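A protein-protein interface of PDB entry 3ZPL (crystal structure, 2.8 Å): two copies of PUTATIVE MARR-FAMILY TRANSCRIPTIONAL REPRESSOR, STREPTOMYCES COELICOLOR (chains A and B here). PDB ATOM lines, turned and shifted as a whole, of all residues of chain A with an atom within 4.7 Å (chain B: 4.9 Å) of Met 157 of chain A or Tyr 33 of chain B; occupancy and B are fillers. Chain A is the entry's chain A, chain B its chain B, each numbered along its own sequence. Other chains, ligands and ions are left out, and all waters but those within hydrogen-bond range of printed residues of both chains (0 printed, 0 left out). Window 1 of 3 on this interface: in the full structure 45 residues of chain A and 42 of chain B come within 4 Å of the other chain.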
ATOM      1  N   TYR A  33      22.617  -2.082  29.534  1.00  0.00           N
ATOM      2  CA  TYR A  33      22.858  -3.518  29.359  1.00  0.00           C
ATOM      3  C   TYR A  33      21.835  -4.127  28.397  1.00  0.00           C
ATOM      4  O   TYR A  33      22.198  -4.717  27.389  1.00  0.00           O
ATOM      5  CB  TYR A  33      22.832  -4.282  30.672  1.00  0.00           C
ATOM      6  CG  TYR A  33      22.911  -5.770  30.448  1.00  0.00           C
ATOM      7  CD1 TYR A  33      24.123  -6.388  30.159  1.00  0.00           C
ATOM      8  CD2 TYR A  33      21.760  -6.562  30.475  1.00  0.00           C
ATOM      9  CE1 TYR A  33      24.201  -7.751  29.924  1.00  0.00           C
ATOM     10  CE2 TYR A  33      21.824  -7.924  30.237  1.00  0.00           C
ATOM     11  CZ  TYR A  33      23.047  -8.516  29.960  1.00  0.00           C
ATOM     12  OH  TYR A  33      23.135  -9.877  29.727  1.00  0.00           O
ATOM     13  N   ALA A  37      22.858  -5.820  24.737  1.00  0.00           N
ATOM     14  CA  ALA A  37      22.617  -7.239  24.514  1.00  0.00           C
ATOM     15  C   ALA A  37      21.642  -7.469  23.375  1.00  0.00           C
ATOM     16  O   ALA A  37      21.860  -8.345  22.532  1.00  0.00           O
ATOM     17  CB  ALA A  37      22.104  -7.887  25.789  1.00  0.00           C
ATOM     18  N   LEU A  40      23.454  -6.551  20.114  1.00  0.00           N
ATOM     19  CA  LEU A  40      24.439  -7.568  19.758  1.00  0.00           C
ATOM     20  C   LEU A  40      23.784  -8.840  19.182  1.00  0.00           C
ATOM     21  O   LEU A  40      24.158  -9.278  18.093  1.00  0.00           O
ATOM     22  CB  LEU A  40      25.300  -7.958  20.958  1.00  0.00           C
ATOM     23  CG  LEU A  40      26.730  -7.453  20.960  1.00  0.00           C
ATOM     24  CD1 LEU A  40      27.434  -7.930  22.224  1.00  0.00           C
ATOM     25  CD2 LEU A  40      27.500  -7.900  19.714  1.00  0.00           C
ATOM     26  N   LEU A 153      34.939  -6.599  32.106  1.00  0.00           N
ATOM     27  CA  LEU A 153      33.765  -7.272  31.533  1.00  0.00           C
ATOM     28  C   LEU A 153      33.690  -8.748  31.919  1.00  0.00           C
ATOM     29  O   LEU A 153      32.646  -9.227  32.364  1.00  0.00           O
ATOM     30  CB  LEU A 153      33.809  -7.181  30.009  1.00  0.00           C
ATOM     31  CG  LEU A 153      32.709  -7.844  29.174  1.00  0.00           C
ATOM     32  CD1 LEU A 153      31.337  -7.438  29.655  1.00  0.00           C
ATOM     33  CD2 LEU A 153      32.855  -7.512  27.697  1.00  0.00           C
ATOM     34  N   GLY A 154      34.802  -9.460  31.736  1.00  0.00           N
ATOM     35  CA  GLY A 154      34.859 -10.895  32.004  1.00  0.00           C
ATOM     36  C   GLY A 154      34.681 -11.225  33.469  1.00  0.00           C
ATOM     37  O   GLY A 154      33.990 -12.180  33.811  1.00  0.00           O
ATOM     38  N   GLU A 155      35.300 -10.428  34.340  1.00  0.00           N
ATOM     39  CA  GLU A 155      35.125 -10.596  35.765  1.00  0.00           C
ATOM     40  C   GLU A 155      33.651 -10.438  36.110  1.00  0.00           C
ATOM     41  O   GLU A 155      33.085 -11.227  36.879  1.00  0.00           O
ATOM     42  CB  GLU A 155      35.982  -9.592  36.510  1.00  0.00           C
ATOM     43  N   ILE A 156      33.017  -9.452  35.489  1.00  0.00           N
ATOM     44  CA  ILE A 156      31.625  -9.121  35.781  1.00  0.00           C
ATOM     45  C   ILE A 156      30.648 -10.198  35.302  1.00  0.00           C
ATOM     46  O   ILE A 156      29.789 -10.639  36.052  1.00  0.00           O
ATOM     47  CB  ILE A 156      31.244  -7.744  35.181  1.00  0.00           C
ATOM     48  CG1 ILE A 156      31.934  -6.637  35.968  1.00  0.00           C
ATOM     49  CG2 ILE A 156      29.735  -7.541  35.221  1.00  0.00           C
ATOM     50  CD1 ILE A 156      31.947  -5.296  35.282  1.00  0.00           C
ATOM     51  N   MET A 157      30.765 -10.608  34.049  1.00  0.00           N
ATOM     52  CA  MET A 157      29.819 -11.564  33.505  1.00  0.00           C
ATOM     53  C   MET A 157      29.982 -12.912  34.196  1.00  0.00           C
ATOM     54  O   MET A 157      28.998 -13.576  34.474  1.00  0.00           O
ATOM     55  CB  MET A 157      29.964 -11.672  31.992  1.00  0.00           C
ATOM     56  CG  MET A 157      29.665 -10.376  31.237  1.00  0.00           C
ATOM     57  SD  MET A 157      28.085  -9.598  31.623  1.00  0.00           S
ATOM     58  CE  MET A 157      26.891 -10.477  30.626  1.00  0.00           C
ATOM     59  N   ARG A 158      31.227 -13.305  34.489  1.00  0.00           N
ATOM     60  CA  ARG A 158      31.516 -14.560  35.161  1.00  0.00           C
ATOM     61  C   ARG A 158      30.802 -14.684  36.504  1.00  0.00           C
ATOM     62  O   ARG A 158      30.254 -15.743  36.830  1.00  0.00           O
ATOM     63  CB  ARG A 158      33.030 -14.711  35.296  1.00  0.00           C
ATOM     64  CG  ARG A 158      33.497 -16.074  35.782  1.00  0.00           C
ATOM     65  CD  ARG A 158      34.744 -16.508  34.984  1.00  0.00           C
ATOM     66  NE  ARG A 158      35.694 -15.389  34.751  1.00  0.00           N
ATOM     67  CZ  ARG A 158      36.115 -14.916  33.559  1.00  0.00           C
ATOM     68  NH1 ARG A 158      35.670 -15.374  32.375  1.00  0.00           N
ATOM     69  NH2 ARG A 158      36.997 -13.914  33.560  1.00  0.00           N
ATOM     70  N   ILE A 159      30.731 -13.586  37.250  1.00  0.00           N
ATOM     71  CA  ILE A 159      29.965 -13.559  38.507  1.00  0.00           C
ATOM     72  C   ILE A 159      28.466 -13.762  38.264  1.00  0.00           C
ATOM     73  O   ILE A 159      27.803 -14.564  38.947  1.00  0.00           O
ATOM     74  CB  ILE A 159      30.106 -12.211  39.236  1.00  0.00           C
ATOM     75  CG1 ILE A 159      31.561 -11.946  39.644  1.00  0.00           C
ATOM     76  CG2 ILE A 159      29.205 -12.185  40.471  1.00  0.00           C
ATOM     77  CD1 ILE A 159      31.878 -10.474  39.836  1.00  0.00           C
ATOM     78  N   VAL A 160      27.935 -13.001  37.304  1.00  0.00           N
ATOM     79  CA  VAL A 160      26.528 -13.086  36.918  1.00  0.00           C
ATOM     80  C   VAL A 160      26.183 -14.515  36.499  1.00  0.00           C
ATOM     81  O   VAL A 160      25.162 -15.056  36.917  1.00  0.00           O
ATOM     82  CB  VAL A 160      26.196 -12.096  35.775  1.00  0.00           C
ATOM     83  CG1 VAL A 160      24.829 -12.378  35.175  1.00  0.00           C
ATOM     84  CG2 VAL A 160      26.264 -10.664  36.284  1.00  0.00           C
ATOM     85  N   ALA A 161      27.037 -15.118  35.685  1.00  0.00           N
ATOM     86  CA  ALA A 161      26.816 -16.485  35.236  1.00  0.00           C
ATOM     87  C   ALA A 161      26.898 -17.456  36.408  1.00  0.00           C
ATOM     88  O   ALA A 161      25.962 -18.229  36.646  1.00  0.00           O
ATOM     89  CB  ALA A 161      27.818 -16.870  34.157  1.00  0.00           C
ATOM     90  N   VAL B  29      36.662 -14.052  28.147  1.00  0.00           N
ATOM     91  CA  VAL B  29      35.786 -12.908  28.389  1.00  0.00           C
ATOM     92  C   VAL B  29      34.482 -13.078  27.604  1.00  0.00           C
ATOM     93  O   VAL B  29      33.388 -13.046  28.173  1.00  0.00           O
ATOM     94  CB  VAL B  29      36.473 -11.583  27.980  1.00  0.00           C
ATOM     95  CG1 VAL B  29      35.479 -10.433  27.965  1.00  0.00           C
ATOM     96  CG2 VAL B  29      37.625 -11.273  28.919  1.00  0.00           C
ATOM     97  N   TRP B  30      34.618 -13.271  26.297  1.00  0.00           N
ATOM     98  CA  TRP B  30      33.472 -13.431  25.409  1.00  0.00           C
ATOM     99  C   TRP B  30      32.586 -14.589  25.825  1.00  0.00           C
ATOM    100  O   TRP B  30      31.373 -14.453  25.894  1.00  0.00           O
ATOM    101  CB  TRP B  30      33.966 -13.646  23.985  1.00  0.00           C
ATOM    102  CG  TRP B  30      32.897 -13.783  22.969  1.00  0.00           C
ATOM    103  CD1 TRP B  30      32.695 -14.846  22.122  1.00  0.00           C
ATOM    104  CD2 TRP B  30      31.884 -12.824  22.662  1.00  0.00           C
ATOM    105  NE1 TRP B  30      31.613 -14.598  21.310  1.00  0.00           N
ATOM    106  CE2 TRP B  30      31.098 -13.363  21.618  1.00  0.00           C
ATOM    107  CE3 TRP B  30      31.570 -11.558  23.154  1.00  0.00           C
ATOM    108  CZ2 TRP B  30      30.009 -12.677  21.068  1.00  0.00           C
ATOM    109  CZ3 TRP B  30      30.489 -10.878  22.599  1.00  0.00           C
ATOM    110  CH2 TRP B  30      29.721 -11.446  21.570  1.00  0.00           C
ATOM    111  N   ARG B  31      33.193 -15.732  26.107  1.00  0.00           N
ATOM    112  CA  ARG B  31      32.429 -16.918  26.472  1.00  0.00           C
ATOM    113  C   ARG B  31      31.598 -16.577  27.724  1.00  0.00           C
ATOM    114  O   ARG B  31      30.376 -16.782  27.729  1.00  0.00           O
ATOM    115  CB  ARG B  31      33.312 -18.205  26.535  1.00  0.00           C
ATOM    116  CG  ARG B  31      32.928 -19.198  27.590  1.00  0.00           C
ATOM    117  CD  ARG B  31      31.490 -19.737  27.544  1.00  0.00           C
ATOM    118  NE  ARG B  31      31.381 -21.046  28.206  1.00  0.00           N
ATOM    119  CZ  ARG B  31      30.240 -21.714  28.387  1.00  0.00           C
ATOM    120  NH1 ARG B  31      29.086 -21.218  27.942  1.00  0.00           N
ATOM    121  NH2 ARG B  31      30.257 -22.892  29.008  1.00  0.00           N
ATOM    122  N   SER B  32      32.218 -15.977  28.744  1.00  0.00           N
ATOM    123  CA  SER B  32      31.489 -15.697  29.979  1.00  0.00           C
ATOM    124  C   SER B  32      30.403 -14.635  29.781  1.00  0.00           C
ATOM    125  O   SER B  32      29.362 -14.682  30.444  1.00  0.00           O
ATOM    126  CB  SER B  32      32.440 -15.337  31.124  1.00  0.00           C
ATOM    127  OG  SER B  32      33.125 -14.126  30.864  1.00  0.00           O
ATOM    128  N   TYR B  33      30.612 -13.714  28.851  1.00  0.00           N
ATOM    129  CA  TYR B  33      29.527 -12.832  28.446  1.00  0.00           C
ATOM    130  C   TYR B  33      28.358 -13.643  27.893  1.00  0.00           C
ATOM    131  O   TYR B  33      27.231 -13.515  28.377  1.00  0.00           O
ATOM    132  CB  TYR B  33      29.962 -11.798  27.405  1.00  0.00           C
ATOM    133  CG  TYR B  33      28.775 -11.020  26.877  1.00  0.00           C
ATOM    134  CD1 TYR B  33      28.212  -9.978  27.612  1.00  0.00           C
ATOM    135  CD2 TYR B  33      28.193 -11.346  25.657  1.00  0.00           C
ATOM    136  CE1 TYR B  33      27.106  -9.269  27.140  1.00  0.00           C
ATOM    137  CE2 TYR B  33      27.091 -10.650  25.172  1.00  0.00           C
ATOM    138  CZ  TYR B  33      26.549  -9.609  25.914  1.00  0.00           C
ATOM    139  OH  TYR B  33      25.457  -8.920  25.434  1.00  0.00           O
ATOM    140  N   ILE B  34      28.621 -14.462  26.874  1.00  0.00           N
ATOM    141  CA  ILE B  34      27.566 -15.234  26.221  1.00  0.00           C
ATOM    142  C   ILE B  34      26.738 -16.010  27.242  1.00  0.00           C
ATOM    143  O   ILE B  34      25.515 -15.977  27.194  1.00  0.00           O
ATOM    144  CB  ILE B  34      28.116 -16.229  25.171  1.00  0.00           C
ATOM    145  CG1 ILE B  34      28.902 -15.519  24.068  1.00  0.00           C
ATOM    146  CG2 ILE B  34      26.978 -17.011  24.520  1.00  0.00           C
ATOM    147  CD1 ILE B  34      28.096 -14.498  23.293  1.00  0.00           C
ATOM    148  N   GLU B  35      27.405 -16.711  28.154  1.00  0.00           N
ATOM    149  CA  GLU B  35      26.709 -17.532  29.141  1.00  0.00           C
ATOM    150  C   GLU B  35      25.814 -16.702  29.994  1.00  0.00           C
ATOM    151  O   GLU B  35      24.614 -16.967  30.136  1.00  0.00           O
ATOM    152  CB  GLU B  35      27.699 -18.209  30.063  1.00  0.00           C
ATOM    153  N   ALA B  36      26.409 -15.676  30.574  1.00  0.00           N
ATOM    154  CA  ALA B  36      25.688 -14.800  31.478  1.00  0.00           C
ATOM    155  C   ALA B  36      24.432 -14.306  30.810  1.00  0.00           C
ATOM    156  O   ALA B  36      23.326 -14.450  31.353  1.00  0.00           O
ATOM    157  CB  ALA B  36      26.577 -13.634  31.873  1.00  0.00           C
ATOM    158  N   ALA B  37      24.602 -13.708  29.633  1.00  0.00           N
ATOM    159  CA  ALA B  37      23.468 -13.131  28.908  1.00  0.00           C
ATOM    160  C   ALA B  37      22.397 -14.172  28.630  1.00  0.00           C
ATOM    161  O   ALA B  37      21.199 -13.910  28.823  1.00  0.00           O
ATOM    162  CB  ALA B  37      23.919 -12.505  27.612  1.00  0.00           C
ATOM    163  N   THR B  38      22.813 -15.354  28.187  1.00  0.00           N
ATOM    164  CA  THR B  38      21.857 -16.398  27.853  1.00  0.00           C
ATOM    165  C   THR B  38      21.132 -16.880  29.100  1.00  0.00           C
ATOM    166  O   THR B  38      19.956 -17.243  29.022  1.00  0.00           O
ATOM    167  CB  THR B  38      22.534 -17.594  27.135  1.00  0.00           C
ATOM    168  OG1 THR B  38      23.309 -17.119  26.025  1.00  0.00           O
ATOM    169  CG2 THR B  38      21.492 -18.599  26.637  1.00  0.00           C
ATOM    170  N   MET B 157      28.704  -1.248  28.467  1.00  0.00           N
ATOM    171  CA  MET B 157      27.582  -1.598  27.605  1.00  0.00           C
ATOM    172  C   MET B 157      27.175  -0.410  26.737  1.00  0.00           C
ATOM    173  O   MET B 157      26.891  -0.583  25.564  1.00  0.00           O
ATOM    174  CB  MET B 157      26.410  -2.139  28.416  1.00  0.00           C
ATOM    175  CG  MET B 157      26.725  -3.428  29.171  1.00  0.00           C
ATOM    176  SD  MET B 157      27.383  -4.777  28.155  1.00  0.00           S
ATOM    177  CE  MET B 157      27.775  -5.924  29.465  1.00  0.00           C
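The guanidinium group of Arg 158 of chain A is in hydrogen-bond range of the side-chain hydroxyl of Ser 32 of chain B.
Printed residues of chain B within 4 Å of Leu 40 of chain A: Tyr 33 (3.9 Å). Of the printed residues of chain B, Arg 158 of chain A touches Ser 32. Arg 31 of chain B touches none of the printed residues of chain A. Of chain A, only Ala 37, Leu 40 and Met 157 come within 4 Å of Tyr 33 of chain B. Printed residues of chain A within 4 Å of Ala 36 of chain B: Met 157 (3.4 Å), Val 160 (3.9 Å) and Ala 161 (3.9999 Å). Of the printed residues of chain A, Ala 37 of chain B touches Tyr 33 (3.4 Å). Of the printed residues of chain A, Met 157 of chain B touches Tyr 33 and Leu 153. The nearest residue of chain A that does not touch Tyr 33 of chain B is Tyr 33 of chain A (4.3 Å). The nearest printed residue of chain A that does not touch Ala 37 of chain B is Met 157 of chain A (4.1 Å).
O of Val 29 of chain B lies within hydrogen-bond range of OG of Ser 32 of chain B, 2.9 Å away. NH2 of Arg 158 of chain A sits close to O of Gly 154 of chain A (3.5 Å).
Hydrophobic or aromatic side chains of chain A that line the printed part of chain B: Tyr 33, Ala 37, Leu 40, Leu 153, Met 157, Val 160 and Ala 161. Hydrophobic or aromatic side chains of chain B within 4 Å of the printed part of chain A: Val 29, Tyr 33, Ala 36, Ala 37 and Met 157. Among the printed residues, 14 pairs touch across the chains.
Among the printed residues, pairs that only touch across the chains: Met 157 of chain A with Tyr 33 of chain B, Tyr 33 of chain A with Ala 37 of chain B, Met 157 of chain A with Ala 36 of chain B, Ala 37 of chain A with Tyr 33 of chain B, Met 157 of chain A with Ser 32 of chain B, Gly 154 of chain A with Ser 32 of chain B, Tyr 33 of chain A with Met 157 of chain B, Leu 153 of chain A with Met 157 of chain B, Leu 40 of chain A with Tyr 33 of chain B, Leu 153 of chain A with Val 29 of chain B, Val 160 of chain A with Ala 36 of chain B, Gly 154 of chain A with Val 29 of chain B and Ala 161 of chain A with Ala 36 of chain B.
Tyr 33 of chain A touches Ala 37 of chain B, and with the chains exchanged Ala 37 of chain A touches Tyr 33 of chain B. Tyr 33 of chain A touches Met 157 of chain B, and with the chains exchanged Met 157 of chain A touches Tyr 33 of chain B. Positions printed for both chains: 33, 37 and 157. Of the 14 pairs that touch across the chains among the printed residues, 4 have their exchanged pair printed and touching as well.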
